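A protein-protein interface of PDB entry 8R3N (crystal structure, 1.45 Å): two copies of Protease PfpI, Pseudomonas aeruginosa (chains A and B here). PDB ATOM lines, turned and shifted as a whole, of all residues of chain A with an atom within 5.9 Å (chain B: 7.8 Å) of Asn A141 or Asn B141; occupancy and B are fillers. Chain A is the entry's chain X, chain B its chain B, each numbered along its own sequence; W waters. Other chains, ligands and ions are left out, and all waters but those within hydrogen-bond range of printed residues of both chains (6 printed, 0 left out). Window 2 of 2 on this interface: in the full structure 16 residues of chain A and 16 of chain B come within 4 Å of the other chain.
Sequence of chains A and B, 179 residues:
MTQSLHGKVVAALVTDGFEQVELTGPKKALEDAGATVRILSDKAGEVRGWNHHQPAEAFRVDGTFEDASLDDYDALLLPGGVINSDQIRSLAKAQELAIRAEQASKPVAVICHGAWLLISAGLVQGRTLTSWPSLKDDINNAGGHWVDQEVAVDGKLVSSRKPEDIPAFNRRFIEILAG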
ATOM      1  N   ILE A 119       2.186 -27.818  -1.017  1.00  0.00           N
ATOM      2  CA  ILE A 119       3.306 -27.767  -1.968  1.00  0.00           C
ATOM      3  C   ILE A 119       4.317 -28.865  -1.666  1.00  0.00           C
ATOM      4  O   ILE A 119       4.745 -29.614  -2.554  1.00  0.00           O
ATOM      5  CB  ILE A 119       3.999 -26.393  -1.900  1.00  0.00           C
ATOM      6  CG1 ILE A 119       3.139 -25.281  -2.490  1.00  0.00           C
ATOM      7  CG2 ILE A 119       5.356 -26.427  -2.610  1.00  0.00           C
ATOM      8  CD1 ILE A 119       3.708 -23.889  -2.213  1.00  0.00           C
ATOM      9  N   LYS A 136       2.209 -16.952  -3.612  1.00  0.00           N
ATOM     10  CA  LYS A 136       1.778 -17.082  -5.017  1.00  0.00           C
ATOM     11  C   LYS A 136       2.902 -17.686  -5.872  1.00  0.00           C
ATOM     12  O   LYS A 136       2.631 -18.588  -6.658  1.00  0.00           O
ATOM     13  CB  LYS A 136       1.273 -15.725  -5.525  1.00  0.00           C
ATOM     14  CG  LYS A 136       1.209 -15.601  -7.045  1.00  0.00           C
ATOM     15  CD  LYS A 136       0.675 -14.282  -7.559  1.00  0.00           C
ATOM     16  CE  LYS A 136       0.352 -14.368  -9.036  1.00  0.00           C
ATOM     17  NZ  LYS A 136      -0.198 -13.104  -9.573  1.00  0.00           N
ATOM     18  N   ASP A 137       4.116 -17.165  -5.712  1.00  0.00           N
ATOM     19  CA  ASP A 137       5.203 -17.664  -6.548  1.00  0.00           C
ATOM     20  C   ASP A 137       5.501 -19.116  -6.246  1.00  0.00           C
ATOM     21  O   ASP A 137       5.709 -19.912  -7.166  1.00  0.00           O
ATOM     22  CB  ASP A 137       6.477 -16.837  -6.358  1.00  0.00           C
ATOM     23  CG  ASP A 137       6.346 -15.447  -6.902  1.00  0.00           C
ATOM     24  OD1 ASP A 137       5.384 -15.168  -7.645  1.00  0.00           O
ATOM     25  OD2 ASP A 137       7.196 -14.620  -6.568  1.00  0.00           O
ATOM     26  N   ASP A 138       5.476 -19.483  -4.964  1.00  0.00           N
ATOM     27  CA  ASP A 138       5.778 -20.859  -4.588  1.00  0.00           C
ATOM     28  C   ASP A 138       4.736 -21.814  -5.136  1.00  0.00           C
ATOM     29  O   ASP A 138       5.072 -22.904  -5.616  1.00  0.00           O
ATOM     30  CB  ASP A 138       5.864 -20.976  -3.067  1.00  0.00           C
ATOM     31  CG  ASP A 138       6.985 -20.156  -2.489  1.00  0.00           C
ATOM     32  OD1 ASP A 138       8.001 -19.928  -3.197  1.00  0.00           O
ATOM     33  OD2 ASP A 138       6.825 -19.688  -1.346  1.00  0.00           O
ATOM     34  N   ILE A 139       3.467 -21.417  -5.075  1.00  0.00           N
ATOM     35  CA  ILE A 139       2.406 -22.265  -5.610  1.00  0.00           C
ATOM     36  C   ILE A 139       2.516 -22.383  -7.125  1.00  0.00           C
ATOM     37  O   ILE A 139       2.405 -23.476  -7.687  1.00  0.00           O
ATOM     38  CB  ILE A 139       1.021 -21.769  -5.157  1.00  0.00           C
ATOM     39  CG1 ILE A 139       0.845 -21.950  -3.646  1.00  0.00           C
ATOM     40  CG2 ILE A 139      -0.057 -22.450  -5.951  1.00  0.00           C
ATOM     41  CD1 ILE A 139      -0.308 -21.179  -3.032  1.00  0.00           C
ATOM     42  N   ASN A 140       2.750 -21.265  -7.810  1.00  0.00           N
ATOM     43  CA  ASN A 140       2.883 -21.325  -9.260  1.00  0.00           C
ATOM     44  C   ASN A 140       4.117 -22.113  -9.665  1.00  0.00           C
ATOM     45  O   ASN A 140       4.079 -22.896 -10.622  1.00  0.00           O
ATOM     46  CB  ASN A 140       2.924 -19.918  -9.834  1.00  0.00           C
ATOM     47  CG  ASN A 140       1.538 -19.337 -10.049  1.00  0.00           C
ATOM     48  OD1 ASN A 140       0.544 -20.068 -10.143  1.00  0.00           O
ATOM     49  ND2 ASN A 140       1.469 -18.012 -10.145  1.00  0.00           N
ATOM     50  N   ASN A 141       5.216 -21.942  -8.934  1.00  0.00           N
ATOM     51  CA  ASN A 141       6.429 -22.690  -9.249  1.00  0.00           C
ATOM     52  C   ASN A 141       6.248 -24.181  -8.981  1.00  0.00           C
ATOM     53  O   ASN A 141       6.882 -25.014  -9.643  1.00  0.00           O
ATOM     54  CB  ASN A 141       7.607 -22.138  -8.446  1.00  0.00           C
ATOM     55  CG  ASN A 141       8.066 -20.774  -8.938  1.00  0.00           C
ATOM     56  OD1 ASN A 141       7.821 -20.387 -10.086  1.00  0.00           O
ATOM     57  ND2 ASN A 141       8.701 -20.019  -8.050  1.00  0.00           N
ATOM     58  N   ALA A 142       5.425 -24.537  -8.001  1.00  0.00           N
ATOM     59  CA  ALA A 142       5.168 -25.939  -7.701  1.00  0.00           C
ATOM     60  C   ALA A 142       4.232 -26.598  -8.705  1.00  0.00           C
ATOM     61  O   ALA A 142       3.982 -27.800  -8.592  1.00  0.00           O
ATOM     62  CB  ALA A 142       4.593 -26.083  -6.294  1.00  0.00           C
ATOM     63  N   GLY A 143       3.720 -25.853  -9.677  1.00  0.00           N
ATOM     64  CA  GLY A 143       2.763 -26.371 -10.628  1.00  0.00           C
ATOM     65  C   GLY A 143       1.322 -26.049 -10.325  1.00  0.00           C
ATOM     66  O   GLY A 143       0.436 -26.495 -11.069  1.00  0.00           O
ATOM     67  N   GLY A 144       1.049 -25.283  -9.263  1.00  0.00           N
ATOM     68  CA  GLY A 144      -0.317 -24.912  -8.953  1.00  0.00           C
ATOM     69  C   GLY A 144      -0.853 -23.828  -9.874  1.00  0.00           C
ATOM     70  O   GLY A 144      -0.140 -23.166 -10.609  1.00  0.00           O
ATOM     71  N   ARG B  89       9.915 -10.482   0.193  1.00  0.00           N
ATOM     72  CA  ARG B  89       9.986 -11.120  -1.119  1.00  0.00           C
ATOM     73  C   ARG B  89       9.042 -10.475  -2.135  1.00  0.00           C
ATOM     74  O   ARG B  89       9.286 -10.561  -3.342  1.00  0.00           O
ATOM     75  CB  ARG B  89       9.717 -12.624  -0.998  1.00  0.00           C
ATOM     76  CG  ARG B  89       8.240 -12.965  -0.787  1.00  0.00           C
ATOM     77  CD  ARG B  89       8.055 -14.446  -0.606  1.00  0.00           C
ATOM     78  NE  ARG B  89       8.350 -15.209  -1.813  1.00  0.00           N
ATOM     79  CZ  ARG B  89       8.175 -16.522  -1.879  1.00  0.00           C
ATOM     80  NH1 ARG B  89       7.691 -17.194  -0.856  1.00  0.00           N
ATOM     81  NH2 ARG B  89       8.473 -17.166  -3.005  1.00  0.00           N
ATOM     82  N   ILE B 119      13.867 -15.904  -5.087  1.00  0.00           N
ATOM     83  CA  ILE B 119      12.890 -16.693  -5.835  1.00  0.00           C
ATOM     84  C   ILE B 119      11.896 -15.784  -6.533  1.00  0.00           C
ATOM     85  O   ILE B 119      11.659 -15.903  -7.741  1.00  0.00           O
ATOM     86  CB  ILE B 119      12.168 -17.692  -4.915  1.00  0.00           C
ATOM     87  CG1 ILE B 119      13.114 -18.809  -4.471  1.00  0.00           C
ATOM     88  CG2 ILE B 119      10.937 -18.223  -5.630  1.00  0.00           C
ATOM     89  CD1 ILE B 119      12.620 -19.532  -3.262  1.00  0.00           C
ATOM     90  N   SER B 120      11.301 -14.866  -5.776  1.00  0.00           N
ATOM     91  CA  SER B 120      10.294 -13.972  -6.332  1.00  0.00           C
ATOM     92  C   SER B 120      10.873 -13.006  -7.354  1.00  0.00           C
ATOM     93  O   SER B 120      10.139 -12.539  -8.231  1.00  0.00           O
ATOM     94  CB  SER B 120       9.565 -13.251  -5.199  1.00  0.00           C
ATOM     95  OG  SER B 120       8.793 -14.197  -4.469  1.00  0.00           O
ATOM     96  N   GLY B 122      12.998 -13.933  -9.548  1.00  0.00           N
ATOM     97  CA  GLY B 122      13.390 -14.747 -10.680  1.00  0.00           C
ATOM     98  C   GLY B 122      14.867 -15.054 -10.741  1.00  0.00           C
ATOM     99  O   GLY B 122      15.382 -15.400 -11.807  1.00  0.00           O
ATOM    100  N   VAL B 124      16.787 -17.309  -8.769  1.00  0.00           N
ATOM    101  CA  VAL B 124      17.360 -18.597  -8.377  1.00  0.00           C
ATOM    102  C   VAL B 124      17.391 -19.594  -9.522  1.00  0.00           C
ATOM    103  O   VAL B 124      17.947 -20.691  -9.364  1.00  0.00           O
ATOM    104  CB  VAL B 124      16.710 -19.209  -7.121  1.00  0.00           C
ATOM    105  CG1 VAL B 124      16.644 -18.193  -6.012  1.00  0.00           C
ATOM    106  CG2 VAL B 124      15.353 -19.748  -7.457  1.00  0.00           C
ATOM    107  N   GLN B 125      16.843 -19.239 -10.676  1.00  0.00           N
ATOM    108  CA  GLN B 125      16.799 -20.142 -11.810  1.00  0.00           C
ATOM    109  C   GLN B 125      18.215 -20.524 -12.241  1.00  0.00           C
ATOM    110  O   GLN B 125      19.056 -19.652 -12.482  1.00  0.00           O
ATOM    111  CB  GLN B 125      16.081 -19.420 -12.940  1.00  0.00           C
ATOM    112  CG  GLN B 125      15.895 -20.276 -14.135  1.00  0.00           C
ATOM    113  CD  GLN B 125      14.733 -21.231 -13.951  1.00  0.00           C
ATOM    114  OE1 GLN B 125      14.927 -22.434 -13.761  1.00  0.00           O
ATOM    115  NE2 GLN B 125      13.514 -20.703 -14.020  1.00  0.00           N
ATOM    116  N   LEU B 135      12.870 -24.079   2.866  1.00  0.00           N
ATOM    117  CA  LEU B 135      12.765 -23.476   1.547  1.00  0.00           C
ATOM    118  C   LEU B 135      13.219 -24.410   0.433  1.00  0.00           C
ATOM    119  O   LEU B 135      13.121 -24.034  -0.741  1.00  0.00           O
ATOM    120  CB  LEU B 135      13.613 -22.203   1.507  1.00  0.00           C
ATOM    121  CG  LEU B 135      12.913 -20.900   1.910  1.00  0.00           C
ATOM    122  CD1 LEU B 135      12.888 -20.794   3.422  1.00  0.00           C
ATOM    123  CD2 LEU B 135      13.600 -19.658   1.297  1.00  0.00           C
ATOM    124  N   LYS B 136      13.732 -25.600   0.774  1.00  0.00           N
ATOM    125  CA  LYS B 136      14.255 -26.528  -0.225  1.00  0.00           C
ATOM    126  C   LYS B 136      13.322 -26.690  -1.411  1.00  0.00           C
ATOM    127  O   LYS B 136      13.750 -26.619  -2.568  1.00  0.00           O
ATOM    128  CB  LYS B 136      14.468 -27.904   0.403  1.00  0.00           C
ATOM    129  CG  LYS B 136      15.063 -28.878  -0.584  1.00  0.00           C
ATOM    130  CD  LYS B 136      15.124 -30.282  -0.012  1.00  0.00           C
ATOM    131  CE  LYS B 136      15.535 -31.298  -1.070  1.00  0.00           C
ATOM    132  NZ  LYS B 136      15.230 -32.696  -0.638  1.00  0.00           N
ATOM    133  N   ASP B 137      12.043 -26.959  -1.137  1.00  0.00           N
ATOM    134  CA  ASP B 137      11.099 -27.229  -2.212  1.00  0.00           C
ATOM    135  C   ASP B 137      10.822 -25.977  -3.038  1.00  0.00           C
ATOM    136  O   ASP B 137      10.687 -26.054  -4.262  1.00  0.00           O
ATOM    137  CB  ASP B 137       9.805 -27.794  -1.631  1.00  0.00           C
ATOM    138  CG  ASP B 137      10.004 -29.150  -0.967  1.00  0.00           C
ATOM    139  OD1 ASP B 137      10.876 -29.908  -1.419  1.00  0.00           O
ATOM    140  OD2 ASP B 137       9.273 -29.459  -0.002  1.00  0.00           O
ATOM    141  N   ASP B 138      10.740 -24.814  -2.387  1.00  0.00           N
ATOM    142  CA  ASP B 138      10.527 -23.571  -3.121  1.00  0.00           C
ATOM    143  C   ASP B 138      11.711 -23.254  -4.036  1.00  0.00           C
ATOM    144  O   ASP B 138      11.527 -22.813  -5.174  1.00  0.00           O
ATOM    145  CB  ASP B 138      10.264 -22.422  -2.141  1.00  0.00           C
ATOM    146  CG  ASP B 138       8.981 -22.631  -1.321  1.00  0.00           C
ATOM    147  OD1 ASP B 138       8.075 -23.333  -1.811  1.00  0.00           O
ATOM    148  OD2 ASP B 138       8.872 -22.081  -0.200  1.00  0.00           O
ATOM    149  N   ILE B 139      12.935 -23.481  -3.559  1.00  0.00           N
ATOM    150  CA  ILE B 139      14.124 -23.220  -4.372  1.00  0.00           C
ATOM    151  C   ILE B 139      14.180 -24.179  -5.559  1.00  0.00           C
ATOM    152  O   ILE B 139      14.368 -23.760  -6.711  1.00  0.00           O
ATOM    153  CB  ILE B 139      15.390 -23.265  -3.494  1.00  0.00           C
ATOM    154  CG1 ILE B 139      15.415 -22.014  -2.606  1.00  0.00           C
ATOM    155  CG2 ILE B 139      16.646 -23.348  -4.344  1.00  0.00           C
ATOM    156  CD1 ILE B 139      16.385 -22.052  -1.452  1.00  0.00           C
ATOM    157  N   ASN B 140      13.950 -25.475  -5.304  1.00  0.00           N
ATOM    158  CA  ASN B 140      13.953 -26.433  -6.406  1.00  0.00           C
ATOM    159  C   ASN B 140      12.806 -26.172  -7.378  1.00  0.00           C
ATOM    160  O   ASN B 140      12.993 -26.243  -8.599  1.00  0.00           O
ATOM    161  CB  ASN B 140      13.930 -27.865  -5.873  1.00  0.00           C
ATOM    162  CG  ASN B 140      15.268 -28.294  -5.286  1.00  0.00           C
ATOM    163  OD1 ASN B 140      16.325 -27.834  -5.713  1.00  0.00           O
ATOM    164  ND2 ASN B 140      15.230 -29.199  -4.312  1.00  0.00           N
ATOM    165  N   ASN B 141      11.616 -25.842  -6.865  1.00  0.00           N
ATOM    166  CA  ASN B 141      10.480 -25.642  -7.760  1.00  0.00           C
ATOM    167  C   ASN B 141      10.687 -24.428  -8.648  1.00  0.00           C
ATOM    168  O   ASN B 141      10.144 -24.364  -9.758  1.00  0.00           O
ATOM    169  CB  ASN B 141       9.187 -25.487  -6.957  1.00  0.00           C
ATOM    170  CG  ASN B 141       8.711 -26.812  -6.391  1.00  0.00           C
ATOM    171  OD1 ASN B 141       9.149 -27.879  -6.825  1.00  0.00           O
ATOM    172  ND2 ASN B 141       7.823 -26.751  -5.418  1.00  0.00           N
ATOM    173  N   ALA B 142      11.484 -23.475  -8.184  1.00  0.00           N
ATOM    174  CA  ALA B 142      11.777 -22.270  -8.935  1.00  0.00           C
ATOM    175  C   ALA B 142      12.953 -22.454  -9.885  1.00  0.00           C
ATOM    176  O   ALA B 142      13.484 -21.460 -10.393  1.00  0.00           O
ATOM    177  CB  ALA B 142      12.032 -21.111  -7.965  1.00  0.00           C
ATOM    178  N   GLY B 143      13.379 -23.696 -10.123  1.00  0.00           N
ATOM    179  CA  GLY B 143      14.456 -23.970 -11.042  1.00  0.00           C
ATOM    180  C   GLY B 143      15.839 -23.904 -10.439  1.00  0.00           C
ATOM    181  O   GLY B 143      16.824 -24.032 -11.178  1.00  0.00           O
ATOM    182  N   GLY B 144      15.953 -23.670  -9.135  1.00  0.00           N
ATOM    183  CA  GLY B 144      17.237 -23.740  -8.480  1.00  0.00           C
ATOM    184  C   GLY B 144      17.659 -25.169  -8.224  1.00  0.00           C
ATOM    185  O   GLY B 144      16.886 -26.116  -8.397  1.00  0.00           O
ATOM    186  N   HIS B 145      18.917 -25.310  -7.817  1.00  0.00           N
ATOM    187  CA  HIS B 145      19.480 -26.581  -7.382  1.00  0.00           C
ATOM    188  C   HIS B 145      19.777 -26.392  -5.899  1.00  0.00           C
ATOM    189  O   HIS B 145      20.764 -25.752  -5.534  1.00  0.00           O
ATOM    190  CB  HIS B 145      20.739 -26.897  -8.186  1.00  0.00           C
ATOM    191  CG  HIS B 145      21.530 -28.053  -7.655  1.00  0.00           C
ATOM    192  ND1 HIS B 145      22.907 -28.042  -7.563  1.00  0.00           N
ATOM    193  CD2 HIS B 145      21.130 -29.263  -7.194  1.00  0.00           C
ATOM    194  CE1 HIS B 145      23.320 -29.196  -7.065  1.00  0.00           C
ATOM    195  NE2 HIS B 145      22.261 -29.951  -6.827  1.00  0.00           N
ATOM    196  N   TRP B 146      18.922 -26.923  -5.033  1.00  0.00           N
ATOM    197  CA  TRP B 146      19.145 -26.780  -3.601  1.00  0.00           C
ATOM    198  C   TRP B 146      20.201 -27.767  -3.123  1.00  0.00           C
ATOM    199  O   TRP B 146      20.146 -28.955  -3.454  1.00  0.00           O
ATOM    200  CB  TRP B 146      17.847 -27.004  -2.832  1.00  0.00           C
ATOM    201  CG  TRP B 146      17.978 -26.648  -1.386  1.00  0.00           C
ATOM    202  CD1 TRP B 146      17.766 -25.421  -0.827  1.00  0.00           C
ATOM    203  CD2 TRP B 146      18.339 -27.527  -0.308  1.00  0.00           C
ATOM    204  NE1 TRP B 146      17.976 -25.480   0.530  1.00  0.00           N
ATOM    205  CE2 TRP B 146      18.330 -26.759   0.875  1.00  0.00           C
ATOM    206  CE3 TRP B 146      18.686 -28.883  -0.231  1.00  0.00           C
ATOM    207  CZ2 TRP B 146      18.641 -27.302   2.124  1.00  0.00           C
ATOM    208  CZ3 TRP B 146      19.000 -29.422   1.011  1.00  0.00           C
ATOM    209  CH2 TRP B 146      18.973 -28.638   2.172  1.00  0.00           C
HETATM  210  O   HOH W   1       9.069 -21.174  -5.599  1.00  0.00           O
HETATM  211  O   HOH W   2       8.117 -24.105 -12.372  1.00  0.00           O
HETATM  212  O   HOH W   3       9.731 -17.412  -8.998  1.00  0.00           O
HETATM  213  O   HOH W   4       7.319 -29.473  -4.069  1.00  0.00           O
HETATM  214  O   HOH W   5       7.707 -12.517  -8.283  1.00  0.00           O
HETATM  215  O   HOH W   6       7.325 -24.173  -4.475  1.00  0.00           O
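Asn A140 touches none of the printed residues of chain B.
Asn A141 touches just these residues of chain B: Ile B119 (3.8 Å), Asn B141 (3.3 Å) and Ala B142 (3.5 Å).
Of the printed residues of chain B, Ala A142 touches Asn B141.
Of the printed residues of chain A, Asp B138 touches Asp A138 (3.4 Å).
The nearest printed residue of chain A that does not touch Asn B141 is Asp A138 (4.7 Å).
The nearest printed residue of chain B that does not touch Asp A138 is Ile B119 (4.2 Å).
Ile A119 touches Asn B141, and with the chains exchanged Asn A141 touches Ile B119.
Asp A138 touches its own counterpart, Asp B138.
Asn A141 touches its own counterpart, Asn B141.
Asn A141 touches Ala B142, and with the chains exchanged Ala A142 touches Asn B141.
Among the printed residues, merely in contact across the chains: Ile A119 with Asn B141, Asp A137 with Arg B89, Asn A141 with Ile B119, Asn A141 with Ala B142 and Ala A142 with Asn B141.
NE of Arg B89 is in hydrogen-bond range of OG of Ser B120 (2.9 Å).
O of Asp B137 sits close to ND2 of Asn B141 (3.2 Å).
The backbone carbonyl oxygen (O) of Asp A137 lies close to the side-chain amide nitrogen (ND2) of Asn A141 (3.1 Å).
Water W5 bridges the backbone carbonyl oxygen (O) of Ser B120 (2.4 Å) and the side-chain carboxylate (OD2) of Asp A137 (2.8 Å).
Water W1 lies within hydrogen-bond range of ND2 of Asn A141 (2.7 Å), OD1 of Asp A138 (2.9 Å) and O of Asp B138 (3.0 Å).
Water W3 bridges O of Ile B119 (2.8 Å) and ND2 of Asn A141 (3.0 Å).
Water W6 lies within hydrogen-bond range of ND2 of Asn B141 (2.8 Å), O of Asp A138 (2.8 Å) and OD1 of Asp B138 (2.9 Å).
Water W4 lies within hydrogen-bond range of the backbone carbonyl oxygen of Ile A119 (3.0 Å) and the side-chain amide nitrogen of Asn B141 (3.1 Å).
Water W2 lies within hydrogen-bond range of the backbone carbonyl oxygen (O) of Asn A141 (3.1 Å) and the backbone carbonyl oxygen (O) of Asn B141 (3.3 Å).
OD2 of Asp A138 lies within salt-bridge range of NH1 of Arg B89 (2.7 Å).
The side-chain carboxylate of Asp A137 sits at hydrogen-bond distance from the side-chain hydroxyl of Ser B120, at 2.7 Å.
OD2 of Asp A138 lies close to OD2 of Asp B138.
The backbone carbonyl oxygen (O) of Asn B141 lies close to the backbone carbonyl oxygen (O) of Asn A141 (3.3 Å).
Hydrophobic or aromatic side chains of chain B that line the printed part of chain A: Ile B119 and Ala B142.
Along chain A the printed residues that touch a printed residue of chain B span positions 119 to 142.
Among the printed residues, 9 pairs touch across the chains.
Among the printed residues, Asp or Glu carboxylates within 4 Å of a Lys or Arg side-chain nitrogen of the other chain: Asp A138 with Arg B89 (2.7 Å).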
